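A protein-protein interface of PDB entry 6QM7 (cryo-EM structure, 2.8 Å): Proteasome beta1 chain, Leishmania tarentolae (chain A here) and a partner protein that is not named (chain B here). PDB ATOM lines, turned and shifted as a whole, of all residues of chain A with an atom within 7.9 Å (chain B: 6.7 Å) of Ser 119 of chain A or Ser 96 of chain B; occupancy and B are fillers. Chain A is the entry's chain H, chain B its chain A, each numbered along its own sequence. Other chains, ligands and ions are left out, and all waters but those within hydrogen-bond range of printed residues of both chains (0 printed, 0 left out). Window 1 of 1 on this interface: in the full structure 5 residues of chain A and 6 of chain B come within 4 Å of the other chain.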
ATOM      1  N   GLU A 111     -11.067  14.647   7.135  1.00  0.00           N
ATOM      2  CA  GLU A 111     -10.003  14.796   6.110  1.00  0.00           C
ATOM      3  C   GLU A 111      -9.136  15.998   6.452  1.00  0.00           C
ATOM      4  O   GLU A 111      -7.918  15.925   6.223  1.00  0.00           O
ATOM      5  CB  GLU A 111     -10.580  14.947   4.704  1.00  0.00           C
ATOM      6  CG  GLU A 111     -10.913  13.609   4.051  1.00  0.00           C
ATOM      7  CD  GLU A 111     -11.817  13.688   2.825  1.00  0.00           C
ATOM      8  OE1 GLU A 111     -12.876  14.366   2.911  1.00  0.00           O
ATOM      9  OE2 GLU A 111     -11.463  13.088   1.775  1.00  0.00           O
ATOM     10  N   ARG A 112      -9.748  17.072   6.944  1.00  0.00           N
ATOM     11  CA  ARG A 112      -9.036  18.314   7.345  1.00  0.00           C
ATOM     12  C   ARG A 112      -8.132  17.964   8.520  1.00  0.00           C
ATOM     13  O   ARG A 112      -6.941  18.225   8.447  1.00  0.00           O
ATOM     14  CB  ARG A 112     -10.046  19.409   7.698  1.00  0.00           C
ATOM     15  CG  ARG A 112      -9.462  20.785   7.976  1.00  0.00           C
ATOM     16  CD  ARG A 112      -8.813  21.464   6.781  1.00  0.00           C
ATOM     17  NE  ARG A 112      -7.428  21.019   6.602  1.00  0.00           N
ATOM     18  CZ  ARG A 112      -6.574  21.467   5.680  1.00  0.00           C
ATOM     19  NH1 ARG A 112      -5.349  20.965   5.625  1.00  0.00           N
ATOM     20  NH2 ARG A 112      -6.945  22.401   4.815  1.00  0.00           N
ATOM     21  N   VAL A 113      -8.691  17.334   9.541  1.00  0.00           N
ATOM     22  CA  VAL A 113      -7.980  17.026  10.810  1.00  0.00           C
ATOM     23  C   VAL A 113      -6.905  15.984  10.534  1.00  0.00           C
ATOM     24  O   VAL A 113      -5.860  16.080  11.161  1.00  0.00           O
ATOM     25  CB  VAL A 113      -8.954  16.538  11.894  1.00  0.00           C
ATOM     26  CG1 VAL A 113      -8.222  16.035  13.130  1.00  0.00           C
ATOM     27  CG2 VAL A 113      -9.933  17.628  12.270  1.00  0.00           C
ATOM     28  N   SER A 114      -7.172  14.999   9.683  1.00  0.00           N
ATOM     29  CA  SER A 114      -6.190  13.943   9.324  1.00  0.00           C
ATOM     30  C   SER A 114      -4.972  14.612   8.699  1.00  0.00           C
ATOM     31  O   SER A 114      -3.854  14.213   9.046  1.00  0.00           O
ATOM     32  CB  SER A 114      -6.776  12.908   8.402  1.00  0.00           C
ATOM     33  OG  SER A 114      -5.778  12.031   7.907  1.00  0.00           O
ATOM     34  N   ASN A 115      -5.210  15.604   7.840  1.00  0.00           N
ATOM     35  CA  ASN A 115      -4.170  16.338   7.081  1.00  0.00           C
ATOM     36  C   ASN A 115      -3.345  17.198   8.040  1.00  0.00           C
ATOM     37  O   ASN A 115      -2.129  17.231   7.861  1.00  0.00           O
ATOM     38  CB  ASN A 115      -4.791  17.191   5.974  1.00  0.00           C
ATOM     39  CG  ASN A 115      -3.763  17.770   5.028  1.00  0.00           C
ATOM     40  OD1 ASN A 115      -3.184  18.821   5.305  1.00  0.00           O
ATOM     41  ND2 ASN A 115      -3.537  17.094   3.913  1.00  0.00           N
ATOM     42  N   TYR A 116      -3.975  17.877   9.002  1.00  0.00           N
ATOM     43  CA  TYR A 116      -3.276  18.676  10.039  1.00  0.00           C
ATOM     44  C   TYR A 116      -2.414  17.751  10.889  1.00  0.00           C
ATOM     45  O   TYR A 116      -1.257  18.100  11.141  1.00  0.00           O
ATOM     46  CB  TYR A 116      -4.234  19.463  10.939  1.00  0.00           C
ATOM     47  CG  TYR A 116      -4.924  20.648  10.312  1.00  0.00           C
ATOM     48  CD1 TYR A 116      -4.343  21.386   9.288  1.00  0.00           C
ATOM     49  CD2 TYR A 116      -6.161  21.062  10.773  1.00  0.00           C
ATOM     50  CE1 TYR A 116      -4.988  22.473   8.715  1.00  0.00           C
ATOM     51  CE2 TYR A 116      -6.820  22.147  10.214  1.00  0.00           C
ATOM     52  CZ  TYR A 116      -6.233  22.858   9.178  1.00  0.00           C
ATOM     53  OH  TYR A 116      -6.872  23.932   8.624  1.00  0.00           O
ATOM     54  N   LEU A 117      -2.967  16.626  11.320  1.00  0.00           N
ATOM     55  CA  LEU A 117      -2.253  15.632  12.163  1.00  0.00           C
ATOM     56  C   LEU A 117      -1.048  15.064  11.417  1.00  0.00           C
ATOM     57  O   LEU A 117      -0.052  14.773  12.094  1.00  0.00           O
ATOM     58  CB  LEU A 117      -3.204  14.495  12.554  1.00  0.00           C
ATOM     59  CG  LEU A 117      -3.843  14.539  13.942  1.00  0.00           C
ATOM     60  CD1 LEU A 117      -3.737  15.901  14.615  1.00  0.00           C
ATOM     61  CD2 LEU A 117      -5.288  14.087  13.850  1.00  0.00           C
ATOM     62  N   GLY A 118      -1.160  14.846  10.109  1.00  0.00           N
ATOM     63  CA  GLY A 118      -0.064  14.294   9.297  1.00  0.00           C
ATOM     64  C   GLY A 118       1.081  15.284   9.172  1.00  0.00           C
ATOM     65  O   GLY A 118       2.253  14.871   9.316  1.00  0.00           O
ATOM     66  N   SER A 119       0.754  16.548   8.891  1.00  0.00           N
ATOM     67  CA  SER A 119       1.693  17.696   8.852  1.00  0.00           C
ATOM     68  C   SER A 119       2.380  17.833  10.212  1.00  0.00           C
ATOM     69  O   SER A 119       3.602  18.045  10.236  1.00  0.00           O
ATOM     70  CB  SER A 119       0.974  18.969   8.495  1.00  0.00           C
ATOM     71  OG  SER A 119       0.161  18.786   7.349  1.00  0.00           O
ATOM     72  N   TYR A 120       1.596  17.775  11.290  1.00  0.00           N
ATOM     73  CA  TYR A 120       2.056  17.942  12.690  1.00  0.00           C
ATOM     74  C   TYR A 120       3.069  16.851  12.986  1.00  0.00           C
ATOM     75  O   TYR A 120       4.138  17.159  13.522  1.00  0.00           O
ATOM     76  CB  TYR A 120       0.896  17.846  13.687  1.00  0.00           C
ATOM     77  CG  TYR A 120       1.287  18.098  15.124  1.00  0.00           C
ATOM     78  CD1 TYR A 120       1.781  19.335  15.514  1.00  0.00           C
ATOM     79  CD2 TYR A 120       1.177  17.108  16.095  1.00  0.00           C
ATOM     80  CE1 TYR A 120       2.157  19.582  16.827  1.00  0.00           C
ATOM     81  CE2 TYR A 120       1.532  17.345  17.414  1.00  0.00           C
ATOM     82  CZ  TYR A 120       2.040  18.584  17.780  1.00  0.00           C
ATOM     83  OH  TYR A 120       2.418  18.852  19.067  1.00  0.00           O
ATOM     84  N   GLN A 121       2.711  15.617  12.641  1.00  0.00           N
ATOM     85  CA  GLN A 121       3.491  14.397  12.959  1.00  0.00           C
ATOM     86  C   GLN A 121       4.826  14.450  12.226  1.00  0.00           C
ATOM     87  O   GLN A 121       5.820  13.966  12.774  1.00  0.00           O
ATOM     88  CB  GLN A 121       2.718  13.148  12.549  1.00  0.00           C
ATOM     89  CG  GLN A 121       3.348  11.866  13.064  1.00  0.00           C
ATOM     90  CD  GLN A 121       2.534  10.661  12.674  1.00  0.00           C
ATOM     91  OE1 GLN A 121       1.330  10.582  12.945  1.00  0.00           O
ATOM     92  NE2 GLN A 121       3.206   9.710  12.043  1.00  0.00           N
ATOM     93  N   THR A 122       4.817  15.000  11.018  1.00  0.00           N
ATOM     94  CA  THR A 122       6.007  15.137  10.151  1.00  0.00           C
ATOM     95  C   THR A 122       6.972  16.138  10.780  1.00  0.00           C
ATOM     96  O   THR A 122       8.183  15.857  10.769  1.00  0.00           O
ATOM     97  CB  THR A 122       5.591  15.517   8.724  1.00  0.00           C
ATOM     98  OG1 THR A 122       4.962  14.372   8.150  1.00  0.00           O
ATOM     99  CG2 THR A 122       6.753  15.951   7.860  1.00  0.00           C
ATOM    100  N   ASP A 123       6.450  17.225  11.341  1.00  0.00           N
ATOM    101  CA  ASP A 123       7.256  18.408  11.732  1.00  0.00           C
ATOM    102  C   ASP A 123       7.748  18.275  13.180  1.00  0.00           C
ATOM    103  O   ASP A 123       8.808  18.841  13.472  1.00  0.00           O
ATOM    104  CB  ASP A 123       6.506  19.709  11.417  1.00  0.00           C
ATOM    105  CG  ASP A 123       6.064  20.539  12.607  1.00  0.00           C
ATOM    106  OD1 ASP A 123       5.635  19.956  13.619  1.00  0.00           O
ATOM    107  OD2 ASP A 123       6.135  21.773  12.497  1.00  0.00           O
ATOM    108  N   ILE A 124       7.011  17.599  14.059  1.00  0.00           N
ATOM    109  CA  ILE A 124       7.483  17.332  15.451  1.00  0.00           C
ATOM    110  C   ILE A 124       8.404  16.113  15.422  1.00  0.00           C
ATOM    111  O   ILE A 124       9.188  15.955  16.383  1.00  0.00           O
ATOM    112  CB  ILE A 124       6.321  17.178  16.455  1.00  0.00           C
ATOM    113  CG1 ILE A 124       5.555  15.860  16.285  1.00  0.00           C
ATOM    114  CG2 ILE A 124       5.403  18.394  16.392  1.00  0.00           C
ATOM    115  CD1 ILE A 124       4.436  15.646  17.289  1.00  0.00           C
ATOM    116  N   GLY A 125       8.312  15.293  14.370  1.00  0.00           N
ATOM    117  CA  GLY A 125       9.109  14.062  14.214  1.00  0.00           C
ATOM    118  C   GLY A 125       8.886  13.111  15.380  1.00  0.00           C
ATOM    119  O   GLY A 125       9.890  12.620  15.947  1.00  0.00           O
ATOM    120  N   VAL A 128       1.672  11.334  17.317  1.00  0.00           N
ATOM    121  CA  VAL A 128       0.616  12.299  17.723  1.00  0.00           C
ATOM    122  C   VAL A 128      -0.121  11.678  18.902  1.00  0.00           C
ATOM    123  O   VAL A 128      -0.353  10.457  18.857  1.00  0.00           O
ATOM    124  CB  VAL A 128      -0.326  12.607  16.551  1.00  0.00           C
ATOM    125  CG1 VAL A 128      -1.424  13.586  16.937  1.00  0.00           C
ATOM    126  CG2 VAL A 128       0.451  13.119  15.348  1.00  0.00           C
ATOM    127  N   VAL B  69       9.980  15.013   4.466  1.00  0.00           N
ATOM    128  CA  VAL B  69       9.021  15.992   3.877  1.00  0.00           C
ATOM    129  C   VAL B  69       7.616  15.416   4.040  1.00  0.00           C
ATOM    130  O   VAL B  69       6.713  16.131   4.477  1.00  0.00           O
ATOM    131  CB  VAL B  69       9.354  16.272   2.404  1.00  0.00           C
ATOM    132  CG1 VAL B  69       8.303  17.141   1.746  1.00  0.00           C
ATOM    133  CG2 VAL B  69      10.731  16.891   2.260  1.00  0.00           C
ATOM    134  N   THR B  70       7.452  14.164   3.645  1.00  0.00           N
ATOM    135  CA  THR B  70       6.272  13.322   3.932  1.00  0.00           C
ATOM    136  C   THR B  70       6.788  11.947   4.324  1.00  0.00           C
ATOM    137  O   THR B  70       7.946  11.636   4.060  1.00  0.00           O
ATOM    138  CB  THR B  70       5.322  13.301   2.727  1.00  0.00           C
ATOM    139  OG1 THR B  70       6.060  13.153   1.513  1.00  0.00           O
ATOM    140  CG2 THR B  70       4.483  14.560   2.655  1.00  0.00           C
ATOM    141  N   ALA B  91       8.333  22.763   1.470  1.00  0.00           N
ATOM    142  CA  ALA B  91       8.089  21.433   0.857  1.00  0.00           C
ATOM    143  C   ALA B  91       6.993  20.700   1.621  1.00  0.00           C
ATOM    144  O   ALA B  91       6.117  20.113   0.990  1.00  0.00           O
ATOM    145  CB  ALA B  91       9.349  20.614   0.847  1.00  0.00           C
ATOM    146  N   ARG B  92       7.064  20.739   2.943  1.00  0.00           N
ATOM    147  CA  ARG B  92       6.054  20.145   3.849  1.00  0.00           C
ATOM    148  C   ARG B  92       4.712  20.846   3.647  1.00  0.00           C
ATOM    149  O   ARG B  92       3.699  20.136   3.535  1.00  0.00           O
ATOM    150  CB  ARG B  92       6.541  20.268   5.286  1.00  0.00           C
ATOM    151  CG  ARG B  92       7.711  19.355   5.583  1.00  0.00           C
ATOM    152  CD  ARG B  92       8.089  19.434   7.037  1.00  0.00           C
ATOM    153  NE  ARG B  92       9.116  18.459   7.349  1.00  0.00           N
ATOM    154  CZ  ARG B  92       9.882  18.487   8.429  1.00  0.00           C
ATOM    155  NH1 ARG B  92       9.743  19.444   9.333  1.00  0.00           N
ATOM    156  NH2 ARG B  92      10.801  17.556   8.601  1.00  0.00           N
ATOM    157  N   GLU B  93       4.714  22.182   3.634  1.00  0.00           N
ATOM    158  CA  GLU B  93       3.530  23.025   3.322  1.00  0.00           C
ATOM    159  C   GLU B  93       2.949  22.530   1.995  1.00  0.00           C
ATOM    160  O   GLU B  93       1.758  22.172   1.968  1.00  0.00           O
ATOM    161  CB  GLU B  93       3.911  24.505   3.228  1.00  0.00           C
ATOM    162  CG  GLU B  93       2.986  25.452   3.980  1.00  0.00           C
ATOM    163  CD  GLU B  93       3.442  26.914   4.015  1.00  0.00           C
ATOM    164  OE1 GLU B  93       4.673  27.172   4.114  1.00  0.00           O
ATOM    165  OE2 GLU B  93       2.563  27.807   3.944  1.00  0.00           O
ATOM    166  N   GLU B  94       3.793  22.461   0.962  1.00  0.00           N
ATOM    167  CA  GLU B  94       3.420  22.142  -0.444  1.00  0.00           C
ATOM    168  C   GLU B  94       2.806  20.742  -0.525  1.00  0.00           C
ATOM    169  O   GLU B  94       1.867  20.566  -1.310  1.00  0.00           O
ATOM    170  CB  GLU B  94       4.652  22.241  -1.350  1.00  0.00           C
ATOM    171  CG  GLU B  94       4.331  22.185  -2.831  1.00  0.00           C
ATOM    172  CD  GLU B  94       3.376  23.265  -3.330  1.00  0.00           C
ATOM    173  OE1 GLU B  94       2.487  22.939  -4.146  1.00  0.00           O
ATOM    174  OE2 GLU B  94       3.512  24.429  -2.895  1.00  0.00           O
ATOM    175  N   ALA B  95       3.342  19.802   0.258  1.00  0.00           N
ATOM    176  CA  ALA B  95       2.958  18.373   0.305  1.00  0.00           C
ATOM    177  C   ALA B  95       1.649  18.201   1.069  1.00  0.00           C
ATOM    178  O   ALA B  95       0.791  17.457   0.596  1.00  0.00           O
ATOM    179  CB  ALA B  95       4.061  17.569   0.946  1.00  0.00           C
ATOM    180  N   SER B  96       1.537  18.833   2.233  1.00  0.00           N
ATOM    181  CA  SER B  96       0.305  18.877   3.065  1.00  0.00           C
ATOM    182  C   SER B  96      -0.835  19.409   2.202  1.00  0.00           C
ATOM    183  O   SER B  96      -1.875  18.754   2.137  1.00  0.00           O
ATOM    184  CB  SER B  96       0.498  19.748   4.290  1.00  0.00           C
ATOM    185  OG  SER B  96       1.648  19.356   5.035  1.00  0.00           O
ATOM    186  N   ASP B  97      -0.587  20.551   1.558  1.00  0.00           N
ATOM    187  CA  ASP B  97      -1.542  21.315   0.716  1.00  0.00           C
ATOM    188  C   ASP B  97      -2.009  20.439  -0.441  1.00  0.00           C
ATOM    189  O   ASP B  97      -3.187  20.499  -0.785  1.00  0.00           O
ATOM    190  CB  ASP B  97      -0.893  22.586   0.158  1.00  0.00           C
ATOM    191  CG  ASP B  97      -1.836  23.773   0.059  1.00  0.00           C
ATOM    192  OD1 ASP B  97      -2.782  23.717  -0.775  1.00  0.00           O
ATOM    193  OD2 ASP B  97      -1.618  24.756   0.820  1.00  0.00           O
ATOM    194  N   TYR B  98      -1.095  19.685  -1.029  1.00  0.00           N
ATOM    195  CA  TYR B  98      -1.363  18.802  -2.185  1.00  0.00           C
ATOM    196  C   TYR B  98      -2.254  17.646  -1.726  1.00  0.00           C
ATOM    197  O   TYR B  98      -3.253  17.367  -2.391  1.00  0.00           O
ATOM    198  CB  TYR B  98      -0.035  18.349  -2.792  1.00  0.00           C
ATOM    199  CG  TYR B  98      -0.140  17.458  -3.999  1.00  0.00           C
ATOM    200  CD1 TYR B  98       0.172  17.925  -5.271  1.00  0.00           C
ATOM    201  CD2 TYR B  98      -0.559  16.144  -3.875  1.00  0.00           C
ATOM    202  CE1 TYR B  98       0.079  17.102  -6.391  1.00  0.00           C
ATOM    203  CE2 TYR B  98      -0.648  15.312  -4.978  1.00  0.00           C
ATOM    204  CZ  TYR B  98      -0.330  15.785  -6.243  1.00  0.00           C
ATOM    205  OH  TYR B  98      -0.403  14.928  -7.307  1.00  0.00           O
ATOM    206  N   GLN B  99      -1.888  16.994  -0.620  1.00  0.00           N
ATOM    207  CA  GLN B  99      -2.629  15.848  -0.022  1.00  0.00           C
ATOM    208  C   GLN B  99      -4.049  16.324   0.288  1.00  0.00           C
ATOM    209  O   GLN B  99      -4.991  15.536   0.101  1.00  0.00           O
ATOM    210  CB  GLN B  99      -1.847  15.276   1.171  1.00  0.00           C
ATOM    211  CG  GLN B  99      -2.678  14.564   2.241  1.00  0.00           C
ATOM    212  CD  GLN B  99      -2.840  13.086   1.987  1.00  0.00           C
ATOM    213  OE1 GLN B  99      -1.871  12.324   1.995  1.00  0.00           O
ATOM    214  NE2 GLN B  99      -4.078  12.670   1.761  1.00  0.00           N
ATOM    215  N   TYR B 100      -4.218  17.566   0.723  1.00  0.00           N
ATOM    216  CA  TYR B 100      -5.561  18.082   1.064  1.00  0.00           C
ATOM    217  C   TYR B 100      -6.358  18.334  -0.214  1.00  0.00           C
ATOM    218  O   TYR B 100      -7.545  17.979  -0.258  1.00  0.00           O
ATOM    219  CB  TYR B 100      -5.510  19.342   1.917  1.00  0.00           C
ATOM    220  CG  TYR B 100      -6.897  19.781   2.300  1.00  0.00           C
ATOM    221  CD1 TYR B 100      -7.691  18.979   3.113  1.00  0.00           C
ATOM    222  CD2 TYR B 100      -7.459  20.937   1.776  1.00  0.00           C
ATOM    223  CE1 TYR B 100      -8.988  19.340   3.443  1.00  0.00           C
ATOM    224  CE2 TYR B 100      -8.754  21.309   2.102  1.00  0.00           C
ATOM    225  CZ  TYR B 100      -9.517  20.513   2.941  1.00  0.00           C
ATOM    226  OH  TYR B 100     -10.790  20.876   3.255  1.00  0.00           O
ATOM    227  N   ARG B 101      -5.718  18.930  -1.214  1.00  0.00           N
ATOM    228  CA  ARG B 101      -6.372  19.352  -2.474  1.00  0.00           C
ATOM    229  C   ARG B 101      -6.754  18.111  -3.284  1.00  0.00           C
ATOM    230  O   ARG B 101      -7.851  18.142  -3.854  1.00  0.00           O
ATOM    231  CB  ARG B 101      -5.479  20.342  -3.240  1.00  0.00           C
ATOM    232  CG  ARG B 101      -5.957  20.663  -4.651  1.00  0.00           C
ATOM    233  CD  ARG B 101      -5.186  21.767  -5.355  1.00  0.00           C
ATOM    234  NE  ARG B 101      -5.622  23.096  -4.925  1.00  0.00           N
ATOM    235  CZ  ARG B 101      -5.097  23.828  -3.932  1.00  0.00           C
ATOM    236  NH1 ARG B 101      -4.066  23.397  -3.218  1.00  0.00           N
ATOM    237  NH2 ARG B 101      -5.614  25.015  -3.657  1.00  0.00           N
ATOM    238  N   ILE B 106       1.789  13.720  -2.410  1.00  0.00           N
ATOM    239  CA  ILE B 106       2.471  14.432  -3.523  1.00  0.00           C
ATOM    240  C   ILE B 106       3.546  13.511  -4.097  1.00  0.00           C
ATOM    241  O   ILE B 106       4.385  13.006  -3.359  1.00  0.00           O
ATOM    242  CB  ILE B 106       3.024  15.804  -3.079  1.00  0.00           C
ATOM    243  CG1 ILE B 106       3.451  16.626  -4.299  1.00  0.00           C
ATOM    244  CG2 ILE B 106       4.143  15.681  -2.053  1.00  0.00           C
ATOM    245  CD1 ILE B 106       3.551  18.093  -4.031  1.00  0.00           C
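Of the printed residues of chain B, Arg 112 of chain A touches Tyr 100 (3.4 Å).
Ser 114 of chain A touches none of the printed residues of chain B.
Printed residues of chain B within 4 Å of Ser 119 of chain A: Ser 96 (2.8 Å).
Printed residues of chain B within 4 Å of Thr 122 of chain A: Val 69 (3.4 Å) and Arg 92 (3.5 Å).
Ile 124 of chain A touches none of the printed residues of chain B.
Printed residues of chain A within 4 Å of Val 69 of chain B: Thr 122.
Ala 95 of chain B touches none of the printed residues of chain A.
Of chain A, only Asn 115 (2.9 Å) and Ser 119 (2.8 Å) come within 4 Å of Ser 96 of chain B.
Of the printed residues of chain A, Tyr 100 of chain B touches Arg 112 (3.4 Å) and Asn 115 (3.3 Å).
The nearest printed residue of chain B that does not touch Asn 115 of chain A is Asp 97 of chain B (4.9 Å).
Printed residues of chain B that touch a printed residue of chain A: Val 69, Arg 92, Ser 96, Gln 99 and Tyr 100.
Hydrophobic or aromatic side chains of chain B that line the printed part of chain A: Tyr 100.
Along chain B the printed residues that touch a printed residue of chain A span positions 69 to 100.
The side-chain amide nitrogen (ND2) of Asn 115 of chain A is in hydrogen-bond range of the backbone carbonyl oxygen (O) of Ser 96 of chain B, at 2.9 Å.
OG of Ser 96 of chain B is in hydrogen-bond range of OG of Ser 119 of chain A.
The backbone NH of Tyr 100 of chain B sits close to the side-chain amide nitrogen of Asn 115 of chain A (3.3 Å).
Arg 112 of chain A touches Tyr 100 of chain B (NH2 to CD2, 3.4 Å).
Asn 115 of chain A touches Gln 99 of chain B.
Val 69 of chain B touches Thr 122 of chain A.
Thr 122 of chain A touches Arg 92 of chain B (CG2 to NE, 3.5 Å).
Asp 123 of chain A touches Arg 92 of chain B.
The side-chain hydroxyl (OG) of Ser 96 of chain B lies within hydrogen-bond range of the backbone carbonyl oxygen (O) of Arg 92 of chain B (2.7 Å).
The side-chain amide oxygen (OD1) of Asn 115 of chain A sits at hydrogen-bond distance from the guanidinium group (NH1) of Arg 112 of chain A (3.1 Å).
The backbone carbonyl oxygen of Asn 115 of chain A sits at hydrogen-bond distance from the side-chain hydroxyl of Ser 119 of chain A.
The backbone carbonyl oxygen (O) of Gly 118 of chain A sits at hydrogen-bond distance from the side-chain hydroxyl (OG1) of Thr 122 of chain A (3.0 Å).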
